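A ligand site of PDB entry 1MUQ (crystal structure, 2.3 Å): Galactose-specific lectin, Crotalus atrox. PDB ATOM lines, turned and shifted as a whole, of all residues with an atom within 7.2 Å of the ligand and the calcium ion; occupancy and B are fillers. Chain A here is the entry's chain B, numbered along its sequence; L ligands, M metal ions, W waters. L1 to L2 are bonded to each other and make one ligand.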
ATOM      1  N   ASN A  65     -14.065   9.441  16.356  1.00  0.00           N
ATOM      2  CA  ASN A  65     -14.180   9.932  14.998  1.00  0.00           C
ATOM      3  C   ASN A  65     -12.938   9.470  14.232  1.00  0.00           C
ATOM      4  O   ASN A  65     -11.971   9.004  14.839  1.00  0.00           O
ATOM      5  CB  ASN A  65     -14.298  11.463  14.992  1.00  0.00           C
ATOM      6  CG  ASN A  65     -15.552  11.932  15.721  1.00  0.00           C
ATOM      7  OD1 ASN A  65     -16.641  11.380  15.544  1.00  0.00           O
ATOM      8  ND2 ASN A  65     -15.404  12.966  16.552  1.00  0.00           N
ATOM      9  N   TRP A  92     -19.569  17.802   4.052  1.00  0.00           N
ATOM     10  CA  TRP A  92     -19.555  18.434   5.364  1.00  0.00           C
ATOM     11  C   TRP A  92     -20.802  18.118   6.178  1.00  0.00           C
ATOM     12  O   TRP A  92     -21.893  17.988   5.642  1.00  0.00           O
ATOM     13  CB  TRP A  92     -19.450  19.953   5.230  1.00  0.00           C
ATOM     14  CG  TRP A  92     -18.132  20.439   4.709  1.00  0.00           C
ATOM     15  CD1 TRP A  92     -17.918  21.120   3.543  1.00  0.00           C
ATOM     16  CD2 TRP A  92     -16.860  20.372   5.380  1.00  0.00           C
ATOM     17  NE1 TRP A  92     -16.599  21.492   3.458  1.00  0.00           N
ATOM     18  CE2 TRP A  92     -15.936  21.048   4.565  1.00  0.00           C
ATOM     19  CE3 TRP A  92     -16.427  19.816   6.590  1.00  0.00           C
ATOM     20  CZ2 TRP A  92     -14.583  21.181   4.921  1.00  0.00           C
ATOM     21  CZ3 TRP A  92     -15.098  19.951   6.943  1.00  0.00           C
ATOM     22  CH2 TRP A  92     -14.189  20.626   6.111  1.00  0.00           C
ATOM     23  N   ASP A  93     -20.635  18.026   7.498  1.00  0.00           N
ATOM     24  CA  ASP A  93     -21.756  17.757   8.379  1.00  0.00           C
ATOM     25  C   ASP A  93     -22.486  19.076   8.609  1.00  0.00           C
ATOM     26  O   ASP A  93     -22.009  20.133   8.213  1.00  0.00           O
ATOM     27  CB  ASP A  93     -21.238  17.196   9.711  1.00  0.00           C
ATOM     28  CG  ASP A  93     -22.359  16.700  10.606  1.00  0.00           C
ATOM     29  OD1 ASP A  93     -23.530  16.731  10.163  1.00  0.00           O
ATOM     30  OD2 ASP A  93     -22.064  16.283  11.740  1.00  0.00           O
ATOM     31  N   LYS A  94     -23.660  19.002   9.238  1.00  0.00           N
ATOM     32  CA  LYS A  94     -24.467  20.178   9.505  1.00  0.00           C
ATOM     33  C   LYS A  94     -23.685  21.309  10.186  1.00  0.00           C
ATOM     34  O   LYS A  94     -23.073  21.108  11.233  1.00  0.00           O
ATOM     35  CB  LYS A  94     -25.669  19.797  10.366  1.00  0.00           C
ATOM     36  CG  LYS A  94     -26.644  20.924  10.644  1.00  0.00           C
ATOM     37  CD  LYS A  94     -27.835  20.416  11.453  1.00  0.00           C
ATOM     38  CE  LYS A  94     -28.886  21.510  11.662  1.00  0.00           C
ATOM     39  NZ  LYS A  94     -30.083  20.999  12.375  1.00  0.00           N
ATOM     40  N   ASN A  95     -23.713  22.489   9.571  1.00  0.00           N
ATOM     41  CA  ASN A  95     -23.032  23.681  10.082  1.00  0.00           C
ATOM     42  C   ASN A  95     -21.511  23.627  10.022  1.00  0.00           C
ATOM     43  O   ASN A  95     -20.836  24.474  10.611  1.00  0.00           O
ATOM     44  CB  ASN A  95     -23.478  23.954  11.528  1.00  0.00           C
ATOM     45  CG  ASN A  95     -24.906  24.439  11.609  1.00  0.00           C
ATOM     46  OD1 ASN A  95     -25.481  24.539  12.695  1.00  0.00           O
ATOM     47  ND2 ASN A  95     -25.502  24.744  10.462  1.00  0.00           N
ATOM     48  N   GLN A  96     -20.974  22.652   9.306  1.00  0.00           N
ATOM     49  CA  GLN A  96     -19.527  22.512   9.165  1.00  0.00           C
ATOM     50  C   GLN A  96     -19.114  22.902   7.745  1.00  0.00           C
ATOM     51  O   GLN A  96     -19.882  22.727   6.795  1.00  0.00           O
ATOM     52  CB  GLN A  96     -19.110  21.067   9.448  1.00  0.00           C
ATOM     53  CG  GLN A  96     -19.527  20.534  10.807  1.00  0.00           C
ATOM     54  CD  GLN A  96     -18.980  21.359  11.957  1.00  0.00           C
ATOM     55  OE1 GLN A  96     -18.001  22.090  11.791  1.00  0.00           O
ATOM     56  NE2 GLN A  96     -19.597  21.247  13.118  1.00  0.00           N
ATOM     57  N   PRO A  97     -17.878  23.417   7.578  1.00  0.00           N
ATOM     58  CA  PRO A  97     -16.892  23.657   8.632  1.00  0.00           C
ATOM     59  C   PRO A  97     -17.138  25.010   9.294  1.00  0.00           C
ATOM     60  O   PRO A  97     -17.811  25.867   8.730  1.00  0.00           O
ATOM     61  CB  PRO A  97     -15.576  23.628   7.860  1.00  0.00           C
ATOM     62  CG  PRO A  97     -15.955  24.321   6.599  1.00  0.00           C
ATOM     63  CD  PRO A  97     -17.300  23.710   6.255  1.00  0.00           C
ATOM     64  N   ASP A  98     -16.585  25.204  10.488  1.00  0.00           N
ATOM     65  CA  ASP A  98     -16.796  26.450  11.201  1.00  0.00           C
ATOM     66  C   ASP A  98     -15.534  26.990  11.856  1.00  0.00           C
ATOM     67  O   ASP A  98     -15.514  28.128  12.333  1.00  0.00           O
ATOM     68  CB  ASP A  98     -17.872  26.258  12.277  1.00  0.00           C
ATOM     69  CG  ASP A  98     -17.458  25.258  13.343  1.00  0.00           C
ATOM     70  OD1 ASP A  98     -16.829  24.234  13.005  1.00  0.00           O
ATOM     71  OD2 ASP A  98     -17.777  25.499  14.527  1.00  0.00           O
ATOM     72  N   HIS A  99     -14.473  26.177  11.876  1.00  0.00           N
ATOM     73  CA  HIS A  99     -13.223  26.580  12.506  1.00  0.00           C
ATOM     74  C   HIS A  99     -13.537  26.989  13.939  1.00  0.00           C
ATOM     75  O   HIS A  99     -13.032  28.003  14.426  1.00  0.00           O
ATOM     76  CB  HIS A  99     -12.596  27.793  11.785  1.00  0.00           C
ATOM     77  CG  HIS A  99     -11.974  27.454  10.461  1.00  0.00           C
ATOM     78  ND1 HIS A  99     -11.330  28.403   9.687  1.00  0.00           N
ATOM     79  CD2 HIS A  99     -11.864  26.283   9.796  1.00  0.00           C
ATOM     80  CE1 HIS A  99     -10.856  27.828   8.596  1.00  0.00           C
ATOM     81  NE2 HIS A  99     -11.162  26.538   8.640  1.00  0.00           N
ATOM     82  N   TYR A 100     -14.376  26.209  14.608  1.00  0.00           N
ATOM     83  CA  TYR A 100     -14.786  26.475  15.987  1.00  0.00           C
ATOM     84  C   TYR A 100     -13.624  27.031  16.818  1.00  0.00           C
ATOM     85  O   TYR A 100     -12.516  26.482  16.815  1.00  0.00           O
ATOM     86  CB  TYR A 100     -15.333  25.191  16.625  1.00  0.00           C
ATOM     87  CG  TYR A 100     -16.002  25.371  17.972  1.00  0.00           C
ATOM     88  CD1 TYR A 100     -16.217  24.274  18.812  1.00  0.00           C
ATOM     89  CD2 TYR A 100     -16.425  26.629  18.412  1.00  0.00           C
ATOM     90  CE1 TYR A 100     -16.822  24.421  20.045  1.00  0.00           C
ATOM     91  CE2 TYR A 100     -17.031  26.783  19.659  1.00  0.00           C
ATOM     92  CZ  TYR A 100     -17.236  25.677  20.472  1.00  0.00           C
ATOM     93  OH  TYR A 100     -17.812  25.814  21.705  1.00  0.00           O
ATOM     94  N   GLN A 101     -13.886  28.131  17.515  1.00  0.00           N
ATOM     95  CA  GLN A 101     -12.885  28.794  18.356  1.00  0.00           C
ATOM     96  C   GLN A 101     -11.642  29.168  17.567  1.00  0.00           C
ATOM     97  O   GLN A 101     -10.610  29.525  18.139  1.00  0.00           O
ATOM     98  CB  GLN A 101     -12.477  27.883  19.519  1.00  0.00           C
ATOM     99  CG  GLN A 101     -13.585  27.584  20.496  1.00  0.00           C
ATOM    100  CD  GLN A 101     -13.146  26.633  21.586  1.00  0.00           C
ATOM    101  OE1 GLN A 101     -12.206  26.928  22.335  1.00  0.00           O
ATOM    102  NE2 GLN A 101     -13.798  25.482  21.664  1.00  0.00           N
ATOM    103  N   GLU A 104      -9.889  24.737  14.693  1.00  0.00           N
ATOM    104  CA  GLU A 104     -10.211  23.467  14.028  1.00  0.00           C
ATOM    105  C   GLU A 104      -9.786  23.565  12.562  1.00  0.00           C
ATOM    106  O   GLU A 104     -10.415  24.278  11.782  1.00  0.00           O
ATOM    107  CB  GLU A 104     -11.704  23.201  14.107  1.00  0.00           C
ATOM    108  CG  GLU A 104     -12.202  22.822  15.482  1.00  0.00           C
ATOM    109  CD  GLU A 104     -13.701  22.593  15.517  1.00  0.00           C
ATOM    110  OE1 GLU A 104     -14.192  22.047  16.532  1.00  0.00           O
ATOM    111  OE2 GLU A 104     -14.382  22.969  14.541  1.00  0.00           O
ATOM    112  N   CYS A 106      -8.439  20.437  10.852  1.00  0.00           N
ATOM    113  CA  CYS A 106      -8.262  19.092  10.332  1.00  0.00           C
ATOM    114  C   CYS A 106      -9.615  18.403  10.253  1.00  0.00           C
ATOM    115  O   CYS A 106     -10.463  18.588  11.133  1.00  0.00           O
ATOM    116  CB  CYS A 106      -7.273  18.326  11.211  1.00  0.00           C
ATOM    117  SG  CYS A 106      -5.584  18.990  11.059  1.00  0.00           S
ATOM    118  N   GLU A 108     -12.426  15.265  10.089  1.00  0.00           N
ATOM    119  CA  GLU A 108     -12.722  13.938  10.594  1.00  0.00           C
ATOM    120  C   GLU A 108     -14.099  13.476  10.153  1.00  0.00           C
ATOM    121  O   GLU A 108     -14.979  14.294   9.840  1.00  0.00           O
ATOM    122  CB  GLU A 108     -12.685  13.929  12.124  1.00  0.00           C
ATOM    123  CG  GLU A 108     -13.794  14.773  12.748  1.00  0.00           C
ATOM    124  CD  GLU A 108     -13.634  14.957  14.260  1.00  0.00           C
ATOM    125  OE1 GLU A 108     -14.524  15.607  14.868  1.00  0.00           O
ATOM    126  OE2 GLU A 108     -12.634  14.461  14.829  1.00  0.00           O
ATOM    127  N   VAL A 110     -17.446  12.286  11.098  1.00  0.00           N
ATOM    128  CA  VAL A 110     -18.280  12.373  12.296  1.00  0.00           C
ATOM    129  C   VAL A 110     -18.919  11.034  12.618  1.00  0.00           C
ATOM    130  O   VAL A 110     -19.783  10.539  11.877  1.00  0.00           O
ATOM    131  CB  VAL A 110     -19.387  13.428  12.129  1.00  0.00           C
ATOM    132  CG1 VAL A 110     -20.237  13.506  13.394  1.00  0.00           C
ATOM    133  CG2 VAL A 110     -18.767  14.775  11.793  1.00  0.00           C
ATOM    134  N   LEU A 112     -21.102  10.289  14.798  1.00  0.00           N
ATOM    135  CA  LEU A 112     -22.538  10.388  15.002  1.00  0.00           C
ATOM    136  C   LEU A 112     -23.344  10.518  13.712  1.00  0.00           C
ATOM    137  O   LEU A 112     -24.576  10.430  13.735  1.00  0.00           O
ATOM    138  CB  LEU A 112     -22.872  11.562  15.942  1.00  0.00           C
ATOM    139  CG  LEU A 112     -22.318  11.460  17.372  1.00  0.00           C
ATOM    140  CD1 LEU A 112     -22.870  12.610  18.195  1.00  0.00           C
ATOM    141  CD2 LEU A 112     -22.685  10.116  17.992  1.00  0.00           C
ATOM    142  N   TRP A 118     -18.484  15.158   7.313  1.00  0.00           N
ATOM    143  CA  TRP A 118     -17.213  15.649   7.826  1.00  0.00           C
ATOM    144  C   TRP A 118     -17.320  16.824   8.802  1.00  0.00           C
ATOM    145  O   TRP A 118     -18.287  17.590   8.774  1.00  0.00           O
ATOM    146  CB  TRP A 118     -16.296  16.046   6.685  1.00  0.00           C
ATOM    147  CG  TRP A 118     -16.178  15.039   5.582  1.00  0.00           C
ATOM    148  CD1 TRP A 118     -16.523  13.717   5.632  1.00  0.00           C
ATOM    149  CD2 TRP A 118     -15.658  15.275   4.276  1.00  0.00           C
ATOM    150  NE1 TRP A 118     -16.244  13.115   4.425  1.00  0.00           N
ATOM    151  CE2 TRP A 118     -15.707  14.042   3.574  1.00  0.00           C
ATOM    152  CE3 TRP A 118     -15.142  16.398   3.625  1.00  0.00           C
ATOM    153  CZ2 TRP A 118     -15.269  13.916   2.259  1.00  0.00           C
ATOM    154  CZ3 TRP A 118     -14.704  16.272   2.309  1.00  0.00           C
ATOM    155  CH2 TRP A 118     -14.773  15.028   1.644  1.00  0.00           C
ATOM    156  N   ASN A 119     -16.295  16.952   9.637  1.00  0.00           N
ATOM    157  CA  ASN A 119     -16.239  18.018  10.612  1.00  0.00           C
ATOM    158  C   ASN A 119     -14.808  18.501  10.750  1.00  0.00           C
ATOM    159  O   ASN A 119     -13.899  17.674  10.901  1.00  0.00           O
ATOM    160  CB  ASN A 119     -16.730  17.517  11.980  1.00  0.00           C
ATOM    161  CG  ASN A 119     -16.522  18.546  13.090  1.00  0.00           C
ATOM    162  OD1 ASN A 119     -16.868  19.720  12.941  1.00  0.00           O
ATOM    163  ND2 ASN A 119     -15.969  18.100  14.221  1.00  0.00           N
ATOM    164  N   ASP A 120     -14.592  19.811  10.664  1.00  0.00           N
ATOM    165  CA  ASP A 120     -13.248  20.304  10.854  1.00  0.00           C
ATOM    166  C   ASP A 120     -13.065  20.187  12.357  1.00  0.00           C
ATOM    167  O   ASP A 120     -13.987  20.469  13.133  1.00  0.00           O
ATOM    168  CB  ASP A 120     -13.076  21.732  10.294  1.00  0.00           C
ATOM    169  CG  ASP A 120     -14.041  22.742  10.875  1.00  0.00           C
ATOM    170  OD1 ASP A 120     -15.214  22.404  11.147  1.00  0.00           O
ATOM    171  OD2 ASP A 120     -13.611  23.900  11.031  1.00  0.00           O
ATOM    172  N   GLN A 121     -11.886  19.728  12.770  1.00  0.00           N
ATOM    173  CA  GLN A 121     -11.634  19.470  14.177  1.00  0.00           C
ATOM    174  C   GLN A 121     -10.257  19.954  14.623  1.00  0.00           C
ATOM    175  O   GLN A 121      -9.428  20.333  13.796  1.00  0.00           O
ATOM    176  CB  GLN A 121     -11.759  17.956  14.393  1.00  0.00           C
ATOM    177  CG  GLN A 121     -11.535  17.452  15.799  1.00  0.00           C
ATOM    178  CD  GLN A 121     -12.480  18.088  16.787  1.00  0.00           C
ATOM    179  OE1 GLN A 121     -12.158  19.118  17.378  1.00  0.00           O
ATOM    180  NE2 GLN A 121     -13.654  17.484  16.958  1.00  0.00           N
ATOM    181  N   VAL A 122     -10.026  19.954  15.932  1.00  0.00           N
ATOM    182  CA  VAL A 122      -8.738  20.360  16.475  1.00  0.00           C
ATOM    183  C   VAL A 122      -7.743  19.277  16.071  1.00  0.00           C
ATOM    184  O   VAL A 122      -7.893  18.117  16.437  1.00  0.00           O
ATOM    185  CB  VAL A 122      -8.780  20.499  18.009  1.00  0.00           C
ATOM    186  CG1 VAL A 122      -7.361  20.710  18.554  1.00  0.00           C
ATOM    187  CG2 VAL A 122      -9.663  21.683  18.378  1.00  0.00           C
HETATM  188  C1  LIG L   1     -22.243  19.761  17.355  1.00  0.00           C
HETATM  189  C2  LIG L   1     -23.493  19.011  16.875  1.00  0.00           C
HETATM  190  C3  LIG L   1     -24.588  19.021  17.947  1.00  0.00           C
HETATM  191  C4  LIG L   1     -24.026  18.528  19.279  1.00  0.00           C
HETATM  192  C5  LIG L   1     -22.810  19.368  19.661  1.00  0.00           C
HETATM  193  C6  LIG L   1     -22.181  18.886  20.953  1.00  0.00           C
HETATM  194  O1  LIG L   1     -23.988  19.629  15.699  1.00  0.00           O
HETATM  195  O2  LIG L   1     -25.662  18.187  17.543  1.00  0.00           O
HETATM  196  O3  LIG L   1     -23.634  17.165  19.148  1.00  0.00           O
HETATM  197  O4  LIG L   1     -21.806  19.264  18.630  1.00  0.00           O
HETATM  198  O5  LIG L   1     -20.965  19.557  21.222  1.00  0.00           O
HETATM  199  C1  LG2 L   2     -19.532  20.399  16.806  1.00  0.00           C
HETATM  200  C2  LG2 L   2     -18.293  20.066  15.971  1.00  0.00           C
HETATM  201  C3  LG2 L   2     -17.154  21.034  16.319  1.00  0.00           C
HETATM  202  C4  LG2 L   2     -17.633  22.477  16.185  1.00  0.00           C
HETATM  203  C5  LG2 L   2     -18.895  22.689  17.033  1.00  0.00           C
HETATM  204  C6  LG2 L   2     -19.463  24.087  16.907  1.00  0.00           C
HETATM  205  O1  LG2 L   2     -17.906  18.731  16.233  1.00  0.00           O
HETATM  206  O2  LG2 L   2     -16.062  20.808  15.448  1.00  0.00           O
HETATM  207  O3  LG2 L   2     -17.919  22.750  14.824  1.00  0.00           O
HETATM  208  O4  LG2 L   2     -19.922  21.765  16.615  1.00  0.00           O
HETATM  209  O5  LG2 L   2     -20.735  24.191  17.530  1.00  0.00           O
HETATM  210  S1  LG2 L   2     -20.900  19.417  16.206  1.00  0.00           S
HETATM  211 CA    CA M   1     -16.066  21.923  13.235  1.00  0.00          CA
HETATM  212  O   HOH W   1     -19.319  16.647  15.185  1.00  0.00           O
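Five residues have an atom within 4 Å of the calcium ion: Gln 96, Asp 98, Glu 104, Asn 119 and Asp 120.
The nearest printed residue that does not touch the calcium ion is His 99 (4.7 Å).
Merely in contact with the ligand: Tyr 100 (3.5 Å).
The nearest printed residue that does not touch the ligand is Gln 121 (4.4 Å).
N of Tyr 100 sits close to OD2 of Asp 98, 3.5 Å away.
The side-chain carboxylate (OD2) of Asp 120 is in hydrogen-bond range of the backbone NH (N) of His 99 (2.6 Å).
The side-chain carboxylate (OE2) of Glu 104 sits close to the backbone NH (N) of Tyr 100, at 3.2 Å.
O of Asn 119 is in hydrogen-bond range of N of Glu 108 (2.9 Å).
The calcium ion is bound by OD1 of Asp 120 (2.3 Å), OD1 of Asn 119 (2.4 Å), OE2 of Glu 104 (2.4 Å), OE1 of Gln 96 (2.4 Å), OD1 of Asp 98 (2.4 Å), O2 of LG2 L2 (2.5 Å), O of Asp 120 (2.5 Å) and O3 of LG2 L2 (2.6 Å).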
